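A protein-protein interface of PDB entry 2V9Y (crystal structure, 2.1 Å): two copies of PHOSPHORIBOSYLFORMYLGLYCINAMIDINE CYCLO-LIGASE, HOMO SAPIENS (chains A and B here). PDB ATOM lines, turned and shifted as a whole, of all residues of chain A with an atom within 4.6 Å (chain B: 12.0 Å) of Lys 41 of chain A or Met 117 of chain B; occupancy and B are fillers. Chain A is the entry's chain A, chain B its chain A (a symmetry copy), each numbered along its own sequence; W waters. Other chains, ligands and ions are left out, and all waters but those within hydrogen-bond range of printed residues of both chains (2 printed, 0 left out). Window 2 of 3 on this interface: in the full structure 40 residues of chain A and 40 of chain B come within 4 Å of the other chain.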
ATOM      1  N   THR A  38       3.492 -12.045 -22.461  1.00  0.00           N
ATOM      2  CA  THR A  38       2.786 -12.375 -21.199  1.00  0.00           C
ATOM      3  C   THR A  38       3.168 -13.702 -20.543  1.00  0.00           C
ATOM      4  O   THR A  38       2.565 -14.115 -19.548  1.00  0.00           O
ATOM      5  CB  THR A  38       1.250 -12.233 -21.297  1.00  0.00           C
ATOM      6  OG1 THR A  38       0.759 -13.166 -22.251  1.00  0.00           O
ATOM      7  CG2 THR A  38       0.833 -10.792 -21.693  1.00  0.00           C
ATOM      8  N   LYS A  39       4.199 -14.348 -21.075  1.00  0.00           N
ATOM      9  CA  LYS A  39       4.899 -15.402 -20.346  1.00  0.00           C
ATOM     10  C   LYS A  39       5.314 -14.902 -18.944  1.00  0.00           C
ATOM     11  O   LYS A  39       5.256 -15.650 -17.958  1.00  0.00           O
ATOM     12  CB  LYS A  39       6.117 -15.913 -21.129  1.00  0.00           C
ATOM     13  CG  LYS A  39       6.789 -17.154 -20.454  1.00  0.00           C
ATOM     14  CD  LYS A  39       7.742 -17.866 -21.407  1.00  0.00           C
ATOM     15  CE  LYS A  39       8.154 -19.241 -20.862  1.00  0.00           C
ATOM     16  NZ  LYS A  39       9.133 -19.951 -21.772  1.00  0.00           N
ATOM     17  N   LEU A  40       5.707 -13.631 -18.860  1.00  0.00           N
ATOM     18  CA  LEU A  40       6.062 -12.977 -17.564  1.00  0.00           C
ATOM     19  C   LEU A  40       4.925 -13.004 -16.555  1.00  0.00           C
ATOM     20  O   LEU A  40       5.164 -13.036 -15.363  1.00  0.00           O
ATOM     21  CB  LEU A  40       6.473 -11.506 -17.774  1.00  0.00           C
ATOM     22  CG  LEU A  40       7.695 -11.195 -18.625  1.00  0.00           C
ATOM     23  CD1 LEU A  40       8.018  -9.684 -18.670  1.00  0.00           C
ATOM     24  CD2 LEU A  40       8.919 -11.958 -18.085  1.00  0.00           C
ATOM     25  N   LYS A  41       3.682 -12.984 -17.026  1.00  0.00           N
ATOM     26  CA  LYS A  41       2.532 -13.036 -16.107  1.00  0.00           C
ATOM     27  C   LYS A  41       2.478 -14.380 -15.358  1.00  0.00           C
ATOM     28  O   LYS A  41       2.197 -14.445 -14.161  1.00  0.00           O
ATOM     29  CB  LYS A  41       1.246 -12.791 -16.902  1.00  0.00           C
ATOM     30  CG  LYS A  41       0.251 -12.024 -16.148  1.00  0.00           C
ATOM     31  CD  LYS A  41       0.180 -10.595 -16.662  1.00  0.00           C
ATOM     32  CE  LYS A  41      -0.891  -9.852 -15.871  1.00  0.00           C
ATOM     33  NZ  LYS A  41      -0.358  -9.329 -14.578  1.00  0.00           N
ATOM     34  N   ILE A  42       2.788 -15.462 -16.059  1.00  0.00           N
ATOM     35  CA  ILE A  42       2.897 -16.810 -15.449  1.00  0.00           C
ATOM     36  C   ILE A  42       4.056 -16.887 -14.460  1.00  0.00           C
ATOM     37  O   ILE A  42       3.886 -17.377 -13.335  1.00  0.00           O
ATOM     38  CB  ILE A  42       3.017 -17.925 -16.524  1.00  0.00           C
ATOM     39  CG1 ILE A  42       1.865 -17.798 -17.533  1.00  0.00           C
ATOM     40  CG2 ILE A  42       3.085 -19.344 -15.851  1.00  0.00           C
ATOM     41  CD1 ILE A  42       1.725 -18.982 -18.481  1.00  0.00           C
ATOM     42  N   ALA A  43       5.225 -16.371 -14.852  1.00  0.00           N
ATOM     43  CA  ALA A  43       6.324 -16.231 -13.909  1.00  0.00           C
ATOM     44  C   ALA A  43       5.902 -15.474 -12.633  1.00  0.00           C
ATOM     45  O   ALA A  43       6.217 -15.900 -11.522  1.00  0.00           O
ATOM     46  CB  ALA A  43       7.540 -15.547 -14.588  1.00  0.00           C
ATOM     47  N   GLN A  44       5.175 -14.366 -12.802  1.00  0.00           N
ATOM     48  CA  GLN A  44       4.700 -13.552 -11.656  1.00  0.00           C
ATOM     49  C   GLN A  44       3.616 -14.272 -10.808  1.00  0.00           C
ATOM     50  O   GLN A  44       3.719 -14.302  -9.583  1.00  0.00           O
ATOM     51  CB  GLN A  44       4.249 -12.181 -12.153  1.00  0.00           C
ATOM     52  CG  GLN A  44       5.418 -11.388 -12.816  1.00  0.00           C
ATOM     53  CD  GLN A  44       4.952 -10.340 -13.825  1.00  0.00           C
ATOM     54  OE1 GLN A  44       3.776 -10.048 -13.921  1.00  0.00           O
ATOM     55  NE2 GLN A  44       5.891  -9.810 -14.613  1.00  0.00           N
ATOM     56  N   LEU A  45       2.632 -14.893 -11.466  1.00  0.00           N
ATOM     57  CA  LEU A  45       1.606 -15.713 -10.784  1.00  0.00           C
ATOM     58  C   LEU A  45       2.207 -16.857  -9.935  1.00  0.00           C
ATOM     59  O   LEU A  45       1.839 -17.003  -8.779  1.00  0.00           O
ATOM     60  CB  LEU A  45       0.563 -16.245 -11.785  1.00  0.00           C
ATOM     61  CG  LEU A  45      -0.490 -15.226 -12.268  1.00  0.00           C
ATOM     62  CD1 LEU A  45      -1.193 -15.588 -13.605  1.00  0.00           C
ATOM     63  CD2 LEU A  45      -1.528 -14.910 -11.172  1.00  0.00           C
ATOM     64  N   GLU A 122       4.333  -6.904 -10.533  1.00  0.00           N
ATOM     65  CA  GLU A 122       4.373  -6.956 -12.006  1.00  0.00           C
ATOM     66  C   GLU A 122       5.571  -6.178 -12.521  1.00  0.00           C
ATOM     67  O   GLU A 122       5.901  -5.113 -11.991  1.00  0.00           O
ATOM     68  CB  GLU A 122       3.083  -6.424 -12.671  1.00  0.00           C
ATOM     69  CG  GLU A 122       3.070  -6.728 -14.205  1.00  0.00           C
ATOM     70  CD  GLU A 122       1.922  -6.082 -14.971  1.00  0.00           C
ATOM     71  OE1 GLU A 122       0.772  -6.450 -14.715  1.00  0.00           O
ATOM     72  OE2 GLU A 122       2.180  -5.239 -15.856  1.00  0.00           O
ATOM     73  N   TYR A 123       6.202  -6.736 -13.560  1.00  0.00           N
ATOM     74  CA  TYR A 123       7.308  -6.109 -14.240  1.00  0.00           C
ATOM     75  C   TYR A 123       7.250  -6.435 -15.733  1.00  0.00           C
ATOM     76  O   TYR A 123       6.580  -7.391 -16.156  1.00  0.00           O
ATOM     77  CB  TYR A 123       8.655  -6.563 -13.631  1.00  0.00           C
ATOM     78  CG  TYR A 123       8.902  -8.049 -13.702  1.00  0.00           C
ATOM     79  CD1 TYR A 123       9.449  -8.622 -14.838  1.00  0.00           C
ATOM     80  CD2 TYR A 123       8.594  -8.889 -12.621  1.00  0.00           C
ATOM     81  CE1 TYR A 123       9.692  -9.975 -14.914  1.00  0.00           C
ATOM     82  CE2 TYR A 123       8.844 -10.269 -12.687  1.00  0.00           C
ATOM     83  CZ  TYR A 123       9.378 -10.801 -13.858  1.00  0.00           C
ATOM     84  OH  TYR A 123       9.634 -12.151 -13.975  1.00  0.00           O
ATOM     85  N   ASP A 124       7.964  -5.640 -16.526  1.00  0.00           N
ATOM     86  CA  ASP A 124       8.170  -5.932 -17.940  1.00  0.00           C
ATOM     87  C   ASP A 124       9.669  -5.961 -18.241  1.00  0.00           C
ATOM     88  O   ASP A 124      10.469  -5.343 -17.527  1.00  0.00           O
ATOM     89  CB  ASP A 124       7.488  -4.860 -18.798  1.00  0.00           C
ATOM     90  CG  ASP A 124       7.267  -5.316 -20.240  1.00  0.00           C
ATOM     91  OD1 ASP A 124       7.180  -6.530 -20.485  1.00  0.00           O
ATOM     92  OD2 ASP A 124       7.182  -4.455 -21.134  1.00  0.00           O
ATOM     93  N   ARG A 168      -2.625 -18.475 -21.195  1.00  0.00           N
ATOM     94  CA  ARG A 168      -3.225 -17.983 -19.953  1.00  0.00           C
ATOM     95  C   ARG A 168      -4.758 -17.989 -19.994  1.00  0.00           C
ATOM     96  O   ARG A 168      -5.402 -18.275 -18.989  1.00  0.00           O
ATOM     97  CB  ARG A 168      -2.672 -16.582 -19.599  1.00  0.00           C
ATOM     98  CG  ARG A 168      -1.138 -16.534 -19.289  1.00  0.00           C
ATOM     99  CD  ARG A 168      -0.517 -15.105 -19.485  1.00  0.00           C
ATOM    100  NE  ARG A 168      -1.421 -14.162 -18.866  1.00  0.00           N
ATOM    101  CZ  ARG A 168      -2.087 -13.197 -19.478  1.00  0.00           C
ATOM    102  NH1 ARG A 168      -2.921 -12.500 -18.750  1.00  0.00           N
ATOM    103  NH2 ARG A 168      -1.915 -12.918 -20.773  1.00  0.00           N
ATOM    104  N   LYS B  41       3.438   9.099 -18.061  1.00  0.00           N
ATOM    105  CA  LYS B  41       2.112   9.196 -17.426  1.00  0.00           C
ATOM    106  C   LYS B  41       1.450  10.554 -17.726  1.00  0.00           C
ATOM    107  O   LYS B  41       0.252  10.646 -17.995  1.00  0.00           O
ATOM    108  CB  LYS B  41       2.262   8.972 -15.918  1.00  0.00           C
ATOM    109  CG  LYS B  41       1.131   8.245 -15.338  1.00  0.00           C
ATOM    110  CD  LYS B  41       1.526   6.810 -15.027  1.00  0.00           C
ATOM    111  CE  LYS B  41       0.329   6.108 -14.395  1.00  0.00           C
ATOM    112  NZ  LYS B  41      -0.618   5.593 -15.428  1.00  0.00           N
ATOM    113  N   GLN B  44       0.320  10.511 -21.265  1.00  0.00           N
ATOM    114  CA  GLN B  44      -0.940   9.729 -21.323  1.00  0.00           C
ATOM    115  C   GLN B  44      -2.155  10.491 -20.728  1.00  0.00           C
ATOM    116  O   GLN B  44      -3.212  10.539 -21.353  1.00  0.00           O
ATOM    117  CB  GLN B  44      -0.724   8.362 -20.678  1.00  0.00           C
ATOM    118  CG  GLN B  44       0.360   7.528 -21.429  1.00  0.00           C
ATOM    119  CD  GLN B  44       1.038   6.476 -20.553  1.00  0.00           C
ATOM    120  OE1 GLN B  44       0.606   6.213 -19.448  1.00  0.00           O
ATOM    121  NE2 GLN B  44       2.142   5.908 -21.047  1.00  0.00           N
ATOM    122  N   TYR B  77      11.728  -0.618 -27.794  1.00  0.00           N
ATOM    123  CA  TYR B  77      10.677  -1.576 -27.464  1.00  0.00           C
ATOM    124  C   TYR B  77       9.510  -0.806 -26.802  1.00  0.00           C
ATOM    125  O   TYR B  77       9.654  -0.185 -25.735  1.00  0.00           O
ATOM    126  CB  TYR B  77      11.233  -2.708 -26.590  1.00  0.00           C
ATOM    127  CG  TYR B  77      10.301  -3.869 -26.395  1.00  0.00           C
ATOM    128  CD1 TYR B  77      10.232  -4.927 -27.310  1.00  0.00           C
ATOM    129  CD2 TYR B  77       9.482  -3.912 -25.279  1.00  0.00           C
ATOM    130  CE1 TYR B  77       9.348  -5.986 -27.104  1.00  0.00           C
ATOM    131  CE2 TYR B  77       8.621  -4.948 -25.066  1.00  0.00           C
ATOM    132  CZ  TYR B  77       8.549  -5.972 -25.968  1.00  0.00           C
ATOM    133  OH  TYR B  77       7.668  -6.977 -25.668  1.00  0.00           O
ATOM    134  N   PHE B  78       8.365  -0.872 -27.472  1.00  0.00           N
ATOM    135  CA  PHE B  78       7.157  -0.101 -27.184  1.00  0.00           C
ATOM    136  C   PHE B  78       6.104  -1.093 -26.694  1.00  0.00           C
ATOM    137  O   PHE B  78       5.486  -1.811 -27.488  1.00  0.00           O
ATOM    138  CB  PHE B  78       6.735   0.624 -28.481  1.00  0.00           C
ATOM    139  CG  PHE B  78       5.475   1.485 -28.380  1.00  0.00           C
ATOM    140  CD1 PHE B  78       4.930   1.870 -27.156  1.00  0.00           C
ATOM    141  CD2 PHE B  78       4.883   1.969 -29.558  1.00  0.00           C
ATOM    142  CE1 PHE B  78       3.794   2.672 -27.107  1.00  0.00           C
ATOM    143  CE2 PHE B  78       3.740   2.779 -29.514  1.00  0.00           C
ATOM    144  CZ  PHE B  78       3.191   3.130 -28.281  1.00  0.00           C
ATOM    145  N   SER B  79       5.925  -1.177 -25.376  1.00  0.00           N
ATOM    146  CA  SER B  79       4.945  -2.134 -24.852  1.00  0.00           C
ATOM    147  C   SER B  79       3.710  -1.404 -24.350  1.00  0.00           C
ATOM    148  O   SER B  79       3.818  -0.338 -23.752  1.00  0.00           O
ATOM    149  CB  SER B  79       5.537  -3.047 -23.779  1.00  0.00           C
ATOM    150  OG  SER B  79       6.203  -2.287 -22.823  1.00  0.00           O
ATOM    151  N   CYS B  80       2.529  -1.942 -24.632  1.00  0.00           N
ATOM    152  CA  CYS B  80       1.341  -1.125 -24.398  1.00  0.00           C
ATOM    153  C   CYS B  80       0.072  -1.888 -24.085  1.00  0.00           C
ATOM    154  O   CYS B  80      -0.094  -3.049 -24.492  1.00  0.00           O
ATOM    155  CB  CYS B  80       1.105  -0.179 -25.587  1.00  0.00           C
ATOM    156  SG  CYS B  80       0.906  -1.029 -27.133  1.00  0.00           S
ATOM    157  N   GLY B  81      -0.834  -1.224 -23.365  1.00  0.00           N
ATOM    158  CA  GLY B  81      -2.223  -1.684 -23.312  1.00  0.00           C
ATOM    159  C   GLY B  81      -2.892  -1.359 -24.642  1.00  0.00           C
ATOM    160  O   GLY B  81      -2.209  -0.993 -25.604  1.00  0.00           O
ATOM    161  N   LYS B  82      -4.226  -1.469 -24.700  1.00  0.00           N
ATOM    162  CA  LYS B  82      -4.994  -0.933 -25.838  1.00  0.00           C
ATOM    163  C   LYS B  82      -4.874   0.596 -25.920  1.00  0.00           C
ATOM    164  O   LYS B  82      -5.212   1.319 -24.981  1.00  0.00           O
ATOM    165  CB  LYS B  82      -6.480  -1.340 -25.753  1.00  0.00           C
ATOM    166  CG  LYS B  82      -6.683  -2.855 -25.669  1.00  0.00           C
ATOM    167  CD  LYS B  82      -8.074  -3.235 -25.198  1.00  0.00           C
ATOM    168  CE  LYS B  82      -8.144  -4.738 -24.887  1.00  0.00           C
ATOM    169  NZ  LYS B  82      -7.756  -5.557 -26.081  1.00  0.00           N
ATOM    170  N   LEU B  83      -4.372   1.069 -27.047  1.00  0.00           N
ATOM    171  CA  LEU B  83      -4.125   2.489 -27.272  1.00  0.00           C
ATOM    172  C   LEU B  83      -4.943   2.939 -28.465  1.00  0.00           C
ATOM    173  O   LEU B  83      -5.277   2.141 -29.325  1.00  0.00           O
ATOM    174  CB  LEU B  83      -2.638   2.741 -27.586  1.00  0.00           C
ATOM    175  CG  LEU B  83      -1.568   2.395 -26.549  1.00  0.00           C
ATOM    176  CD1 LEU B  83      -0.223   2.854 -27.042  1.00  0.00           C
ATOM    177  CD2 LEU B  83      -1.859   3.013 -25.204  1.00  0.00           C
ATOM    178  N   THR B 111       6.558  -3.004 -31.300  1.00  0.00           N
ATOM    179  CA  THR B 111       5.373  -2.601 -30.542  1.00  0.00           C
ATOM    180  C   THR B 111       4.692  -3.867 -30.051  1.00  0.00           C
ATOM    181  O   THR B 111       4.327  -4.716 -30.847  1.00  0.00           O
ATOM    182  CB  THR B 111       4.385  -1.811 -31.416  1.00  0.00           C
ATOM    183  OG1 THR B 111       5.025  -0.629 -31.905  1.00  0.00           O
ATOM    184  CG2 THR B 111       3.152  -1.416 -30.612  1.00  0.00           C
ATOM    185  N   ALA B 112       4.517  -4.007 -28.739  1.00  0.00           N
ATOM    186  CA  ALA B 112       3.944  -5.227 -28.216  1.00  0.00           C
ATOM    187  C   ALA B 112       2.731  -4.871 -27.377  1.00  0.00           C
ATOM    188  O   ALA B 112       2.853  -4.339 -26.249  1.00  0.00           O
ATOM    189  CB  ALA B 112       4.991  -6.003 -27.398  1.00  0.00           C
ATOM    190  N   GLU B 113       1.548  -5.151 -27.939  1.00  0.00           N
ATOM    191  CA  GLU B 113       0.303  -4.853 -27.251  1.00  0.00           C
ATOM    192  C   GLU B 113      -0.016  -5.987 -26.323  1.00  0.00           C
ATOM    193  O   GLU B 113      -0.153  -7.124 -26.760  1.00  0.00           O
ATOM    194  CB  GLU B 113      -0.866  -4.611 -28.215  1.00  0.00           C
ATOM    195  CG  GLU B 113      -2.127  -4.168 -27.476  1.00  0.00           C
ATOM    196  CD  GLU B 113      -3.319  -3.926 -28.389  1.00  0.00           C
ATOM    197  OE1 GLU B 113      -3.143  -3.324 -29.477  1.00  0.00           O
ATOM    198  OE2 GLU B 113      -4.441  -4.317 -28.009  1.00  0.00           O
ATOM    199  N   MET B 114      -0.162  -5.668 -25.037  1.00  0.00           N
ATOM    200  CA  MET B 114      -0.446  -6.665 -24.020  1.00  0.00           C
ATOM    201  C   MET B 114      -1.452  -6.096 -23.006  1.00  0.00           C
ATOM    202  O   MET B 114      -1.032  -5.546 -21.971  1.00  0.00           O
ATOM    203  CB  MET B 114       0.871  -7.098 -23.325  1.00  0.00           C
ATOM    204  CG  MET B 114       1.942  -7.700 -24.267  1.00  0.00           C
ATOM    205  SD  MET B 114       3.552  -7.997 -23.458  1.00  0.00           S
ATOM    206  CE  MET B 114       4.267  -6.364 -23.410  1.00  0.00           C
ATOM    207  N   PRO B 115      -2.779  -6.207 -23.307  1.00  0.00           N
ATOM    208  CA  PRO B 115      -3.849  -5.745 -22.412  1.00  0.00           C
ATOM    209  C   PRO B 115      -3.805  -6.267 -20.973  1.00  0.00           C
ATOM    210  O   PRO B 115      -4.286  -5.592 -20.070  1.00  0.00           O
ATOM    211  CB  PRO B 115      -5.138  -6.214 -23.118  1.00  0.00           C
ATOM    212  CG  PRO B 115      -4.759  -6.282 -24.543  1.00  0.00           C
ATOM    213  CD  PRO B 115      -3.341  -6.758 -24.559  1.00  0.00           C
ATOM    214  N   ASP B 116      -3.244  -7.454 -20.757  1.00  0.00           N
ATOM    215  CA  ASP B 116      -3.175  -8.011 -19.406  1.00  0.00           C
ATOM    216  C   ASP B 116      -2.034  -7.467 -18.587  1.00  0.00           C
ATOM    217  O   ASP B 116      -1.934  -7.744 -17.387  1.00  0.00           O
ATOM    218  CB  ASP B 116      -3.101  -9.533 -19.447  1.00  0.00           C
ATOM    219  CG  ASP B 116      -4.413 -10.156 -19.880  1.00  0.00           C
ATOM    220  OD1 ASP B 116      -5.459  -9.489 -19.718  1.00  0.00           O
ATOM    221  OD2 ASP B 116      -4.386 -11.301 -20.402  1.00  0.00           O
ATOM    222  N   MET B 117      -1.191  -6.662 -19.223  1.00  0.00           N
ATOM    223  CA  MET B 117      -0.024  -6.142 -18.575  1.00  0.00           C
ATOM    224  C   MET B 117      -0.181  -4.645 -18.240  1.00  0.00           C
ATOM    225  O   MET B 117       0.436  -4.137 -17.284  1.00  0.00           O
ATOM    226  CB  MET B 117       1.149  -6.388 -19.523  1.00  0.00           C
ATOM    227  CG  MET B 117       2.439  -6.495 -18.874  1.00  0.00           C
ATOM    228  SD  MET B 117       2.730  -8.122 -18.196  1.00  0.00           S
ATOM    229  CE  MET B 117       4.505  -7.931 -18.320  1.00  0.00           C
ATOM    230  N   TYR B 118      -1.007  -3.952 -19.040  1.00  0.00           N
ATOM    231  CA  TYR B 118      -1.161  -2.501 -18.990  1.00  0.00           C
ATOM    232  C   TYR B 118      -2.654  -2.159 -19.120  1.00  0.00           C
ATOM    233  O   TYR B 118      -3.346  -2.757 -19.923  1.00  0.00           O
ATOM    234  CB  TYR B 118      -0.385  -1.813 -20.141  1.00  0.00           C
ATOM    235  CG  TYR B 118       1.110  -1.983 -20.120  1.00  0.00           C
ATOM    236  CD1 TYR B 118       1.912  -1.132 -19.371  1.00  0.00           C
ATOM    237  CD2 TYR B 118       1.728  -3.004 -20.849  1.00  0.00           C
ATOM    238  CE1 TYR B 118       3.318  -1.286 -19.335  1.00  0.00           C
ATOM    239  CE2 TYR B 118       3.109  -3.183 -20.803  1.00  0.00           C
ATOM    240  CZ  TYR B 118       3.898  -2.320 -20.052  1.00  0.00           C
ATOM    241  OH  TYR B 118       5.271  -2.482 -20.008  1.00  0.00           O
ATOM    242  N   PRO B 119      -3.140  -1.167 -18.348  1.00  0.00           N
ATOM    243  CA  PRO B 119      -4.530  -0.709 -18.515  1.00  0.00           C
ATOM    244  C   PRO B 119      -4.677   0.103 -19.834  1.00  0.00           C
ATOM    245  O   PRO B 119      -3.663   0.572 -20.382  1.00  0.00           O
ATOM    246  CB  PRO B 119      -4.756   0.200 -17.295  1.00  0.00           C
ATOM    247  CG  PRO B 119      -3.519   0.149 -16.492  1.00  0.00           C
ATOM    248  CD  PRO B 119      -2.412  -0.380 -17.333  1.00  0.00           C
ATOM    249  N   PRO B 120      -5.923   0.254 -20.347  1.00  0.00           N
ATOM    250  CA  PRO B 120      -6.161   1.040 -21.547  1.00  0.00           C
ATOM    251  C   PRO B 120      -5.468   2.400 -21.501  1.00  0.00           C
ATOM    252  O   PRO B 120      -5.562   3.106 -20.499  1.00  0.00           O
ATOM    253  CB  PRO B 120      -7.695   1.203 -21.537  1.00  0.00           C
ATOM    254  CG  PRO B 120      -8.174  -0.095 -20.952  1.00  0.00           C
ATOM    255  CD  PRO B 120      -7.182  -0.330 -19.827  1.00  0.00           C
ATOM    256  N   GLY B 121      -4.778   2.771 -22.580  1.00  0.00           N
ATOM    257  CA  GLY B 121      -4.129   4.086 -22.625  1.00  0.00           C
ATOM    258  C   GLY B 121      -2.739   4.181 -22.007  1.00  0.00           C
ATOM    259  O   GLY B 121      -2.073   5.209 -22.112  1.00  0.00           O
ATOM    260  N   GLU B 122      -2.285   3.113 -21.371  1.00  0.00           N
ATOM    261  CA  GLU B 122      -0.940   3.138 -20.768  1.00  0.00           C
ATOM    262  C   GLU B 122       0.024   2.321 -21.608  1.00  0.00           C
ATOM    263  O   GLU B 122      -0.338   1.256 -22.119  1.00  0.00           O
ATOM    264  CB  GLU B 122      -0.916   2.630 -19.308  1.00  0.00           C
ATOM    265  CG  GLU B 122       0.468   2.909 -18.634  1.00  0.00           C
ATOM    266  CD  GLU B 122       0.641   2.281 -17.256  1.00  0.00           C
ATOM    267  OE1 GLU B 122      -0.079   2.683 -16.338  1.00  0.00           O
ATOM    268  OE2 GLU B 122       1.528   1.417 -17.090  1.00  0.00           O
ATOM    269  N   TYR B 123       1.248   2.846 -21.734  1.00  0.00           N
ATOM    270  CA  TYR B 123       2.325   2.178 -22.424  1.00  0.00           C
ATOM    271  C   TYR B 123       3.652   2.481 -21.727  1.00  0.00           C
ATOM    272  O   TYR B 123       3.766   3.446 -20.956  1.00  0.00           O
ATOM    273  CB  TYR B 123       2.373   2.607 -23.909  1.00  0.00           C
ATOM    274  CG  TYR B 123       2.584   4.084 -24.125  1.00  0.00           C
ATOM    275  CD1 TYR B 123       3.859   4.623 -24.133  1.00  0.00           C
ATOM    276  CD2 TYR B 123       1.499   4.949 -24.332  1.00  0.00           C
ATOM    277  CE1 TYR B 123       4.068   5.968 -24.341  1.00  0.00           C
ATOM    278  CE2 TYR B 123       1.703   6.321 -24.551  1.00  0.00           C
ATOM    279  CZ  TYR B 123       3.004   6.819 -24.531  1.00  0.00           C
ATOM    280  OH  TYR B 123       3.255   8.161 -24.733  1.00  0.00           O
ATOM    281  N   ASP B 124       4.655   1.655 -22.012  1.00  0.00           N
ATOM    282  CA  ASP B 124       6.026   1.917 -21.587  1.00  0.00           C
ATOM    283  C   ASP B 124       6.949   1.902 -22.807  1.00  0.00           C
ATOM    284  O   ASP B 124       6.637   1.275 -23.827  1.00  0.00           O
ATOM    285  CB  ASP B 124       6.473   0.849 -20.582  1.00  0.00           C
ATOM    286  CG  ASP B 124       7.687   1.288 -19.764  1.00  0.00           C
ATOM    287  OD1 ASP B 124       7.902   2.499 -19.598  1.00  0.00           O
ATOM    288  OD2 ASP B 124       8.433   0.414 -19.284  1.00  0.00           O
ATOM    289  N   LEU B 125       8.096   2.570 -22.670  1.00  0.00           N
ATOM    290  CA  LEU B 125       9.128   2.667 -23.697  1.00  0.00           C
ATOM    291  C   LEU B 125      10.511   2.263 -23.157  1.00  0.00           C
ATOM    292  O   LEU B 125      10.900   2.645 -22.054  1.00  0.00           O
ATOM    293  CB  LEU B 125       9.169   4.099 -24.234  1.00  0.00           C
ATOM    294  CG  LEU B 125       8.002   4.467 -25.166  1.00  0.00           C
ATOM    295  CD1 LEU B 125       7.921   5.995 -25.373  1.00  0.00           C
ATOM    296  CD2 LEU B 125       8.147   3.701 -26.521  1.00  0.00           C
HETATM  297  O   HOH W   1      -5.035 -13.908 -21.609  1.00  0.00           O
HETATM  298  O   HOH W   2       7.058  -8.218 -22.581  1.00  0.00           O
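The guanidinium group (NH1) of Arg 168 of chain A lies within salt-bridge range of the side-chain carboxylate (OD2) of Asp 116 of chain B (2.5 Å). The side-chain carboxylate (OD2) of Asp 124 of chain A lies within hydrogen-bond range of the side-chain hydroxyl (OG) of Ser 79 of chain B, at 2.9 Å. The side-chain carboxylate (OD2) of Asp 124 of chain A lies within hydrogen-bond range of the side-chain hydroxyl (OH) of Tyr 118 of chain B, at 3.0 Å. The backbone carbonyl oxygen (O) of Met 117 of chain B sits close to the side-chain carboxylate (OE2) of Glu 122 of chain A (2.5 Å).
OG of Ser 79 of chain B lies within hydrogen-bond range of OH of Tyr 118 of chain B, 3.0 Å away. NE2 of Gln 44 of chain A lies close to O of Leu 40 of chain A (3.4 Å). The backbone carbonyl oxygen (O) of Ser 79 of chain B sits at hydrogen-bond distance from the backbone NH (N) of Asp 124 of chain B, 2.8 Å away. OG1 of Thr 38 of chain A is in hydrogen-bond range of NH2 of Arg 168 of chain A, at 3.1 Å. The side-chain amide nitrogen (NE2) of Gln 44 of chain A lies within hydrogen-bond range of the backbone carbonyl oxygen (O) of Tyr 123 of chain A (3.0 Å). NZ of Lys 41 of chain A is in salt-bridge range of OE1 of Glu 122 of chain A, 3.1 Å away.
Among the printed residues, merely in contact across the chains: Leu 40 of chain A with Met 117 of chain B, Lys 41 of chain A with Asp 116 of chain B, Lys 41 of chain A with Met 117 of chain B, Tyr 123 of chain A with Met 117 of chain B and Asp 124 of chain A with Met 117 of chain B.
No residue of chain B comes within 4 Å of Thr 38 of chain A. Of chain B, only Asp 116 (2.8 Å) and Met 117 (3.9 Å) come within 4 Å of Lys 41 of chain A. Ile 42 of chain A touches none of the printed residues of chain B. No residue of chain B comes within 4 Å of Leu 45 of chain A. Of the printed residues of chain B, Glu 122 of chain A touches Met 117. Asp 124 of chain A touches three residues of chain B. Of the printed residues of chain A, Ser 79 of chain B touches Asp 124. Of the printed residues of chain A, Asp 116 of chain B touches Lys 41 and Arg 168.
Of the 24 printed residues of chain B, 4 touch a printed residue of chain A. Hydrophobic or aromatic side chains of chain B that line the printed part of chain A: Met 117 and Tyr 118. Hydrophobic or aromatic side chains of chain A within 4 Å of the printed part of chain B: Leu 40. Among the printed residues, Asp or Glu carboxylates within 4 Å of a Lys or Arg side-chain nitrogen of the other chain: Arg 168 of chain A with Asp 116 of chain B.
Positions printed for both chains: 41, 44, 122, 123 and 124. Of the 9 pairs that touch across the chains among the printed residues, none has its exchanged pair printed and touching as well.
Water W2 lies within hydrogen-bond range of the side-chain carboxylate of Asp 124 of chain A, the side-chain hydroxyl of Tyr 77 of chain B and the side-chain sulfur of Met 114 of chain B. Water W1 lies within hydrogen-bond range of OD2 of Asp 116 of chain B and NH2 of Arg 168 of chain A.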
